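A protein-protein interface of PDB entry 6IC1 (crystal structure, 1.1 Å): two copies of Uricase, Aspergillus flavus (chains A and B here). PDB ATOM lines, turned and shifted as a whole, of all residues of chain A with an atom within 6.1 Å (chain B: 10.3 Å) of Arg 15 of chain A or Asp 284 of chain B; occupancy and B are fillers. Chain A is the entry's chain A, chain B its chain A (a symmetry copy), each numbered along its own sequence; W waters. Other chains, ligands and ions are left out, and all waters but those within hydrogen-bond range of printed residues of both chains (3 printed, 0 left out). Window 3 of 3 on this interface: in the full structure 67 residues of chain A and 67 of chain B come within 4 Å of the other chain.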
ATOM      1  N   ASP A  12     -22.590 -29.567 -20.899  1.00  0.00           N
ATOM      2  CA  ASP A  12     -22.138 -29.983 -19.560  1.00  0.00           C
ATOM      3  C   ASP A  12     -20.726 -29.483 -19.318  1.00  0.00           C
ATOM      4  O   ASP A  12     -19.972 -29.150 -20.257  1.00  0.00           O
ATOM      5  CB  ASP A  12     -22.226 -31.502 -19.443  1.00  0.00           C
ATOM      6  CG  ASP A  12     -22.223 -32.084 -18.034  1.00  0.00           C
ATOM      7  OD1 ASP A  12     -22.198 -31.311 -17.059  1.00  0.00           O
ATOM      8  OD2 ASP A  12     -22.270 -33.337 -17.960  1.00  0.00           O
ATOM      9  N   ASN A  13     -20.346 -29.473 -18.065  1.00  0.00           N
ATOM     10  CA  ASN A  13     -18.978 -29.235 -17.637  1.00  0.00           C
ATOM     11  C   ASN A  13     -18.491 -27.850 -18.084  1.00  0.00           C
ATOM     12  O   ASN A  13     -17.317 -27.681 -18.448  1.00  0.00           O
ATOM     13  CB  ASN A  13     -18.045 -30.361 -18.094  1.00  0.00           C
ATOM     14  CG  ASN A  13     -18.405 -31.634 -17.404  1.00  0.00           C
ATOM     15  OD1 ASN A  13     -18.381 -31.651 -16.152  1.00  0.00           O
ATOM     16  ND2 ASN A  13     -18.742 -32.660 -18.140  1.00  0.00           N
ATOM     17  N   VAL A  14     -19.357 -26.848 -17.968  1.00  0.00           N
ATOM     18  CA  VAL A  14     -18.974 -25.465 -18.283  1.00  0.00           C
ATOM     19  C   VAL A  14     -18.405 -24.831 -17.032  1.00  0.00           C
ATOM     20  O   VAL A  14     -19.131 -24.489 -16.083  1.00  0.00           O
ATOM     21  CB  VAL A  14     -20.147 -24.647 -18.814  1.00  0.00           C
ATOM     22  CG1 VAL A  14     -19.698 -23.253 -19.159  1.00  0.00           C
ATOM     23  CG2 VAL A  14     -20.772 -25.318 -20.055  1.00  0.00           C
ATOM     24  N   ARG A  15     -17.084 -24.659 -17.035  1.00  0.00           N
ATOM     25  CA  ARG A  15     -16.401 -24.022 -15.918  1.00  0.00           C
ATOM     26  C   ARG A  15     -16.582 -22.515 -16.001  1.00  0.00           C
ATOM     27  O   ARG A  15     -16.380 -21.929 -17.063  1.00  0.00           O
ATOM     28  CB  ARG A  15     -14.941 -24.406 -15.886  1.00  0.00           C
ATOM     29  CG  ARG A  15     -14.710 -25.915 -15.746  1.00  0.00           C
ATOM     30  CD  ARG A  15     -13.267 -26.279 -15.546  1.00  0.00           C
ATOM     31  NE  ARG A  15     -12.767 -25.733 -14.313  1.00  0.00           N
ATOM     32  CZ  ARG A  15     -11.477 -25.713 -13.932  1.00  0.00           C
ATOM     33  NH1 ARG A  15     -10.544 -26.220 -14.722  1.00  0.00           N
ATOM     34  NH2 ARG A  15     -11.163 -25.139 -12.772  1.00  0.00           N
ATOM     35  N   VAL A  16     -16.931 -21.876 -14.884  1.00  0.00           N
ATOM     36  CA  VAL A  16     -17.186 -20.425 -14.858  1.00  0.00           C
ATOM     37  C   VAL A  16     -16.564 -19.838 -13.605  1.00  0.00           C
ATOM     38  O   VAL A  16     -16.789 -20.328 -12.505  1.00  0.00           O
ATOM     39  CB  VAL A  16     -18.689 -20.117 -14.865  1.00  0.00           C
ATOM     40  CG1 VAL A  16     -18.904 -18.595 -14.943  1.00  0.00           C
ATOM     41  CG2 VAL A  16     -19.430 -20.844 -15.954  1.00  0.00           C
ATOM     42  N   TYR A  17     -15.806 -18.754 -13.793  1.00  0.00           N
ATOM     43  CA  TYR A  17     -15.305 -17.921 -12.678  1.00  0.00           C
ATOM     44  C   TYR A  17     -15.911 -16.553 -12.840  1.00  0.00           C
ATOM     45  O   TYR A  17     -16.014 -16.045 -13.949  1.00  0.00           O
ATOM     46  CB  TYR A  17     -13.775 -17.893 -12.732  1.00  0.00           C
ATOM     47  CG  TYR A  17     -13.083 -16.806 -11.916  1.00  0.00           C
ATOM     48  CD1 TYR A  17     -13.038 -15.512 -12.420  1.00  0.00           C
ATOM     49  CD2 TYR A  17     -12.372 -17.092 -10.763  1.00  0.00           C
ATOM     50  CE1 TYR A  17     -12.326 -14.528 -11.745  1.00  0.00           C
ATOM     51  CE2 TYR A  17     -11.650 -16.117 -10.087  1.00  0.00           C
ATOM     52  CZ  TYR A  17     -11.578 -14.838 -10.625  1.00  0.00           C
ATOM     53  OH  TYR A  17     -10.749 -13.929 -10.004  1.00  0.00           O
ATOM     54  N   GLU A  32     -16.615 -19.571  -8.256  1.00  0.00           N
ATOM     55  CA  GLU A  32     -16.256 -20.513  -9.300  1.00  0.00           C
ATOM     56  C   GLU A  32     -17.280 -21.645  -9.245  1.00  0.00           C
ATOM     57  O   GLU A  32     -17.595 -22.164  -8.170  1.00  0.00           O
ATOM     58  CB  GLU A  32     -14.835 -20.986  -9.201  1.00  0.00           C
ATOM     59  CG  GLU A  32     -14.445 -21.853 -10.334  1.00  0.00           C
ATOM     60  CD  GLU A  32     -12.970 -22.270 -10.440  1.00  0.00           C
ATOM     61  OE1 GLU A  32     -12.128 -21.546  -9.891  1.00  0.00           O
ATOM     62  OE2 GLU A  32     -12.725 -23.347 -11.065  1.00  0.00           O
ATOM     63  N   MET A  33     -17.713 -22.056 -10.432  1.00  0.00           N
ATOM     64  CA  MET A  33     -18.724 -23.103 -10.572  1.00  0.00           C
ATOM     65  C   MET A  33     -18.453 -23.962 -11.793  1.00  0.00           C
ATOM     66  O   MET A  33     -17.614 -23.615 -12.651  1.00  0.00           O
ATOM     67  CB  MET A  33     -20.110 -22.511 -10.648  1.00  0.00           C
ATOM     68  CG  MET A  33     -20.395 -21.553 -11.555  1.00  0.00           C
ATOM     69  SD  MET A  33     -22.045 -20.658 -11.198  1.00  0.00           S
ATOM     70  CE  MET A  33     -21.772 -19.372 -12.406  1.00  0.00           C
ATOM     71  N   THR A  34     -19.138 -25.090 -11.836  1.00  0.00           N
ATOM     72  CA  THR A  34     -19.260 -25.891 -13.049  1.00  0.00           C
ATOM     73  C   THR A  34     -20.737 -26.007 -13.338  1.00  0.00           C
ATOM     74  O   THR A  34     -21.524 -26.381 -12.445  1.00  0.00           O
ATOM     75  CB  THR A  34     -18.597 -27.257 -12.906  1.00  0.00           C
ATOM     76  OG1 THR A  34     -17.247 -27.020 -12.507  1.00  0.00           O
ATOM     77  CG2 THR A  34     -18.653 -27.996 -14.217  1.00  0.00           C
ATOM     78  N   VAL A  35     -21.151 -25.678 -14.559  1.00  0.00           N
ATOM     79  CA  VAL A  35     -22.556 -25.562 -14.952  1.00  0.00           C
ATOM     80  C   VAL A  35     -22.882 -26.570 -16.031  1.00  0.00           C
ATOM     81  O   VAL A  35     -22.116 -26.780 -16.963  1.00  0.00           O
ATOM     82  CB  VAL A  35     -22.865 -24.148 -15.434  1.00  0.00           C
ATOM     83  CG1 VAL A  35     -24.313 -23.973 -15.815  1.00  0.00           C
ATOM     84  CG2 VAL A  35     -22.452 -23.120 -14.408  1.00  0.00           C
ATOM     85  N   TYR A  66     -22.078 -17.880 -20.067  1.00  0.00           N
ATOM     86  CA  TYR A  66     -21.103 -16.805 -19.804  1.00  0.00           C
ATOM     87  C   TYR A  66     -21.781 -15.434 -19.798  1.00  0.00           C
ATOM     88  O   TYR A  66     -21.515 -14.609 -18.947  1.00  0.00           O
ATOM     89  CB  TYR A  66     -19.990 -16.792 -20.845  1.00  0.00           C
ATOM     90  CG  TYR A  66     -19.143 -18.032 -20.982  1.00  0.00           C
ATOM     91  CD1 TYR A  66     -18.813 -18.821 -19.882  1.00  0.00           C
ATOM     92  CD2 TYR A  66     -18.627 -18.365 -22.229  1.00  0.00           C
ATOM     93  CE1 TYR A  66     -18.003 -19.938 -20.046  1.00  0.00           C
ATOM     94  CE2 TYR A  66     -17.835 -19.467 -22.413  1.00  0.00           C
ATOM     95  CZ  TYR A  66     -17.515 -20.251 -21.303  1.00  0.00           C
ATOM     96  OH  TYR A  66     -16.746 -21.369 -21.515  1.00  0.00           O
ATOM     97  N   HIS A 105     -17.688 -24.355  -6.285  1.00  0.00           N
ATOM     98  CA  HIS A 105     -16.377 -24.704  -5.732  1.00  0.00           C
ATOM     99  C   HIS A 105     -15.981 -23.684  -4.673  1.00  0.00           C
ATOM    100  O   HIS A 105     -16.240 -22.494  -4.807  1.00  0.00           O
ATOM    101  CB  HIS A 105     -15.371 -24.721  -6.862  1.00  0.00           C
ATOM    102  CG  HIS A 105     -15.758 -25.623  -7.981  1.00  0.00           C
ATOM    103  ND1 HIS A 105     -15.760 -27.000  -7.810  1.00  0.00           N
ATOM    104  CD2 HIS A 105     -16.185 -25.354  -9.220  1.00  0.00           C
ATOM    105  CE1 HIS A 105     -16.222 -27.509  -8.928  1.00  0.00           C
ATOM    106  NE2 HIS A 105     -16.500 -26.513  -9.840  1.00  0.00           N
ATOM    107  N   PRO B 254     -21.805 -37.766 -24.630  1.00  0.00           N
ATOM    108  CA  PRO B 254     -21.084 -36.487 -24.675  1.00  0.00           C
ATOM    109  C   PRO B 254     -20.571 -36.259 -26.088  1.00  0.00           C
ATOM    110  O   PRO B 254     -20.161 -37.176 -26.794  1.00  0.00           O
ATOM    111  CB  PRO B 254     -19.921 -36.722 -23.709  1.00  0.00           C
ATOM    112  CG  PRO B 254     -19.645 -38.183 -23.780  1.00  0.00           C
ATOM    113  CD  PRO B 254     -21.032 -38.823 -23.940  1.00  0.00           C
ATOM    114  N   ASN B 255     -20.545 -34.993 -26.502  1.00  0.00           N
ATOM    115  CA  ASN B 255     -19.878 -34.600 -27.749  1.00  0.00           C
ATOM    116  C   ASN B 255     -18.507 -34.067 -27.322  1.00  0.00           C
ATOM    117  O   ASN B 255     -18.422 -32.995 -26.751  1.00  0.00           O
ATOM    118  CB  ASN B 255     -20.703 -33.544 -28.470  1.00  0.00           C
ATOM    119  CG  ASN B 255     -20.258 -33.295 -29.880  1.00  0.00           C
ATOM    120  OD1 ASN B 255     -19.340 -33.976 -30.381  1.00  0.00           O
ATOM    121  ND2 ASN B 255     -20.944 -32.374 -30.567  1.00  0.00           N
ATOM    122  N   LYS B 256     -17.481 -34.925 -27.486  1.00  0.00           N
ATOM    123  CA  LYS B 256     -16.137 -34.650 -26.934  1.00  0.00           C
ATOM    124  C   LYS B 256     -15.421 -33.839 -28.038  1.00  0.00           C
ATOM    125  O   LYS B 256     -14.962 -34.435 -29.024  1.00  0.00           O
ATOM    126  CB  LYS B 256     -15.433 -35.958 -26.613  1.00  0.00           C
ATOM    127  CG  LYS B 256     -16.205 -36.802 -25.609  1.00  0.00           C
ATOM    128  CD  LYS B 256     -15.582 -38.158 -25.371  1.00  0.00           C
ATOM    129  CE  LYS B 256     -14.351 -38.110 -24.506  1.00  0.00           C
ATOM    130  NZ  LYS B 256     -13.636 -39.400 -24.488  1.00  0.00           N
ATOM    131  N   HIS B 257     -15.411 -32.544 -27.907  1.00  0.00           N
ATOM    132  CA  HIS B 257     -15.056 -31.683 -29.030  1.00  0.00           C
ATOM    133  C   HIS B 257     -13.555 -31.696 -29.320  1.00  0.00           C
ATOM    134  O   HIS B 257     -12.728 -31.697 -28.408  1.00  0.00           O
ATOM    135  CB  HIS B 257     -15.466 -30.225 -28.715  1.00  0.00           C
ATOM    136  CG  HIS B 257     -16.918 -30.083 -28.349  1.00  0.00           C
ATOM    137  ND1 HIS B 257     -17.956 -30.314 -29.241  1.00  0.00           N
ATOM    138  CD2 HIS B 257     -17.515 -29.789 -27.177  1.00  0.00           C
ATOM    139  CE1 HIS B 257     -19.092 -30.163 -28.557  1.00  0.00           C
ATOM    140  NE2 HIS B 257     -18.875 -29.820 -27.279  1.00  0.00           N
ATOM    141  N   TYR B 258     -13.242 -31.643 -30.610  1.00  0.00           N
ATOM    142  CA  TYR B 258     -11.878 -31.522 -31.123  1.00  0.00           C
ATOM    143  C   TYR B 258     -11.861 -30.243 -31.964  1.00  0.00           C
ATOM    144  O   TYR B 258     -12.519 -30.169 -32.998  1.00  0.00           O
ATOM    145  CB  TYR B 258     -11.460 -32.720 -31.960  1.00  0.00           C
ATOM    146  CG  TYR B 258     -11.165 -33.958 -31.161  1.00  0.00           C
ATOM    147  CD1 TYR B 258     -12.140 -34.599 -30.419  1.00  0.00           C
ATOM    148  CD2 TYR B 258      -9.881 -34.490 -31.112  1.00  0.00           C
ATOM    149  CE1 TYR B 258     -11.845 -35.684 -29.619  1.00  0.00           C
ATOM    150  CE2 TYR B 258      -9.580 -35.616 -30.332  1.00  0.00           C
ATOM    151  CZ  TYR B 258     -10.560 -36.174 -29.557  1.00  0.00           C
ATOM    152  OH  TYR B 258     -10.314 -37.263 -28.749  1.00  0.00           O
ATOM    153  N   PHE B 259     -11.162 -29.225 -31.468  1.00  0.00           N
ATOM    154  CA  PHE B 259     -11.164 -27.918 -32.100  1.00  0.00           C
ATOM    155  C   PHE B 259     -10.047 -27.805 -33.113  1.00  0.00           C
ATOM    156  O   PHE B 259      -8.897 -28.181 -32.870  1.00  0.00           O
ATOM    157  CB  PHE B 259     -11.023 -26.800 -31.091  1.00  0.00           C
ATOM    158  CG  PHE B 259     -12.217 -26.510 -30.212  1.00  0.00           C
ATOM    159  CD1 PHE B 259     -13.441 -27.131 -30.342  1.00  0.00           C
ATOM    160  CD2 PHE B 259     -12.076 -25.538 -29.263  1.00  0.00           C
ATOM    161  CE1 PHE B 259     -14.498 -26.754 -29.537  1.00  0.00           C
ATOM    162  CE2 PHE B 259     -13.129 -25.179 -28.424  1.00  0.00           C
ATOM    163  CZ  PHE B 259     -14.368 -25.798 -28.589  1.00  0.00           C
ATOM    164  N   ALA B 280      -6.921 -29.603 -31.324  1.00  0.00           N
ATOM    165  CA  ALA B 280      -6.865 -29.506 -29.866  1.00  0.00           C
ATOM    166  C   ALA B 280      -8.037 -30.219 -29.272  1.00  0.00           C
ATOM    167  O   ALA B 280      -9.196 -29.709 -29.309  1.00  0.00           O
ATOM    168  CB  ALA B 280      -6.854 -28.051 -29.448  1.00  0.00           C
ATOM    169  N   PRO B 281      -7.882 -31.458 -28.735  1.00  0.00           N
ATOM    170  CA  PRO B 281      -8.977 -32.095 -28.000  1.00  0.00           C
ATOM    171  C   PRO B 281      -9.349 -31.229 -26.803  1.00  0.00           C
ATOM    172  O   PRO B 281      -8.452 -30.818 -26.056  1.00  0.00           O
ATOM    173  CB  PRO B 281      -8.356 -33.440 -27.560  1.00  0.00           C
ATOM    174  CG  PRO B 281      -7.183 -33.659 -28.470  1.00  0.00           C
ATOM    175  CD  PRO B 281      -6.649 -32.238 -28.689  1.00  0.00           C
ATOM    176  N   GLN B 282     -10.652 -30.995 -26.599  1.00  0.00           N
ATOM    177  CA  GLN B 282     -11.128 -30.182 -25.486  1.00  0.00           C
ATOM    178  C   GLN B 282     -11.620 -31.099 -24.364  1.00  0.00           C
ATOM    179  O   GLN B 282     -12.548 -31.885 -24.540  1.00  0.00           O
ATOM    180  CB  GLN B 282     -12.289 -29.288 -25.938  1.00  0.00           C
ATOM    181  CG  GLN B 282     -11.935 -28.392 -27.130  1.00  0.00           C
ATOM    182  CD  GLN B 282     -10.845 -27.405 -26.792  1.00  0.00           C
ATOM    183  OE1 GLN B 282     -11.040 -26.552 -25.915  1.00  0.00           O
ATOM    184  NE2 GLN B 282      -9.714 -27.516 -27.494  1.00  0.00           N
ATOM    185  N   SER B 283     -11.053 -30.949 -23.176  1.00  0.00           N
ATOM    186  CA  SER B 283     -11.497 -31.727 -22.044  1.00  0.00           C
ATOM    187  C   SER B 283     -12.861 -31.302 -21.566  1.00  0.00           C
ATOM    188  O   SER B 283     -13.678 -32.146 -21.158  1.00  0.00           O
ATOM    189  CB  SER B 283     -10.498 -31.666 -20.930  1.00  0.00           C
ATOM    190  OG  SER B 283      -9.244 -32.194 -21.368  1.00  0.00           O
ATOM    191  N   ASP B 284     -13.125 -30.004 -21.573  1.00  0.00           N
ATOM    192  CA  ASP B 284     -14.411 -29.462 -21.165  1.00  0.00           C
ATOM    193  C   ASP B 284     -14.517 -28.100 -21.826  1.00  0.00           C
ATOM    194  O   ASP B 284     -13.516 -27.485 -22.210  1.00  0.00           O
ATOM    195  CB  ASP B 284     -14.554 -29.353 -19.627  1.00  0.00           C
ATOM    196  CG  ASP B 284     -13.442 -28.567 -18.976  1.00  0.00           C
ATOM    197  OD1 ASP B 284     -13.476 -27.343 -19.017  1.00  0.00           O
ATOM    198  OD2 ASP B 284     -12.501 -29.217 -18.461  1.00  0.00           O
ATOM    199  N   PRO B 285     -15.740 -27.539 -21.949  1.00  0.00           N
ATOM    200  CA  PRO B 285     -17.017 -28.203 -21.751  1.00  0.00           C
ATOM    201  C   PRO B 285     -17.244 -29.269 -22.815  1.00  0.00           C
ATOM    202  O   PRO B 285     -16.455 -29.462 -23.720  1.00  0.00           O
ATOM    203  CB  PRO B 285     -18.008 -27.067 -21.853  1.00  0.00           C
ATOM    204  CG  PRO B 285     -17.318 -25.891 -22.118  1.00  0.00           C
ATOM    205  CD  PRO B 285     -15.911 -26.147 -22.412  1.00  0.00           C
ATOM    206  N   ASN B 286     -18.400 -29.940 -22.705  1.00  0.00           N
ATOM    207  CA  ASN B 286     -18.784 -30.914 -23.717  1.00  0.00           C
ATOM    208  C   ASN B 286     -20.289 -30.863 -23.907  1.00  0.00           C
ATOM    209  O   ASN B 286     -21.055 -30.791 -22.963  1.00  0.00           O
ATOM    210  CB  ASN B 286     -18.401 -32.368 -23.347  1.00  0.00           C
ATOM    211  CG  ASN B 286     -18.982 -32.887 -22.066  1.00  0.00           C
ATOM    212  OD1 ASN B 286     -18.434 -32.564 -21.000  1.00  0.00           O
ATOM    213  ND2 ASN B 286     -20.072 -33.642 -22.114  1.00  0.00           N
ATOM    214  N   GLY B 287     -20.709 -30.965 -25.162  1.00  0.00           N
ATOM    215  CA  GLY B 287     -22.110 -31.232 -25.426  1.00  0.00           C
ATOM    216  C   GLY B 287     -22.548 -32.497 -24.693  1.00  0.00           C
ATOM    217  O   GLY B 287     -21.731 -33.426 -24.525  1.00  0.00           O
HETATM  218  O   HOH W   1     -16.048 -32.486 -19.909  1.00  0.00           O
HETATM  219  O   HOH W   2     -15.343 -25.273 -19.177  1.00  0.00           O
HETATM  220  O   HOH W   3     -21.086 -34.956 -19.745  1.00  0.00           O
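Printed residues of chain A that touch a printed residue of chain B: Asp 12, Asn 13, Val 14 and Arg 15.
Hydrophobic or aromatic side chains of chain A within 4 Å of the printed part of chain B: Val 14.
Hydrophobic or aromatic side chains of chain B within 4 Å of the printed part of chain A: Pro 285.
Among the printed residues, no Asp or Glu carboxylate lies within 4 Å of a Lys or Arg side-chain nitrogen of the other chain.
The backbone NH (N) of Asn 13 of chain A sits at hydrogen-bond distance from the backbone carbonyl oxygen (O) of Val 35 of chain A (3.4 Å).
The backbone carbonyl oxygen (O) of Val 14 of chain A lies within hydrogen-bond range of the backbone NH (N) of Val 35 of chain A (2.8 Å).
The side-chain carboxylate (OE2) of Glu 32 of chain A is in salt-bridge range of the guanidinium group (NH2) of Arg 15 of chain A (2.9 Å).
Water W1 lies within hydrogen-bond range of the side-chain amide oxygen of Asn 286 of chain B, the backbone carbonyl oxygen of Ser 283 of chain B and the side-chain amide nitrogen of Asn 13 of chain A.
Water W3 lies within hydrogen-bond range of the side-chain carboxylate of Asp 12 of chain A (2.7 Å) and the side-chain amide nitrogen of Asn 286 of chain B (2.9 Å).
Water W2 lies within hydrogen-bond range of OD1 of Asp 284 of chain B, N of Arg 15 of chain A and O of Asn 13 of chain A.
Of the printed residues of chain B, Asp 12 of chain A touches Pro 285 (3.3 Å) and Asn 286 (2.8 Å).
Val 14 of chain A touches just one residue of chain B: Pro 285.
Arg 15 of chain A touches just one residue of chain B: Asp 284 (3.6 Å).
Val 16 of chain A touches none of the printed residues of chain B.
Gln 282 of chain B touches none of the printed residues of chain A.
Asp 284 of chain B touches just these residues of chain A: Asn 13 (3.4 Å) and Arg 15 (3.6 Å).
Printed residues of chain A within 4 Å of Pro 285 of chain B: Asp 12 (3.3 Å), Asn 13 (3.4 Å) and Val 14 (3.7 Å).
Of the printed residues of chain A, Asn 286 of chain B touches Asp 12 and Asn 13.
O of Asn 286 of chain B lies within hydrogen-bond range of N of Asp 12 of chain A, at 2.8 Å.
The side-chain amide nitrogen (ND2) of Asn 13 of chain A is in hydrogen-bond range of the side-chain amide oxygen (OD1) of Asn 286 of chain B.
Among the printed residues, merely in contact across the chains: Asp 12 of chain A with Pro 285 of chain B (3.3 Å), Asn 13 of chain A with Asp 284 of chain B (3.4 Å), Asn 13 of chain A with Pro 285 of chain B (3.4 Å), Val 14 of chain A with Pro 285 of chain B (3.7 Å) and Arg 15 of chain A with Asp 284 of chain B (3.6 Å).
No position is printed for both chains.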
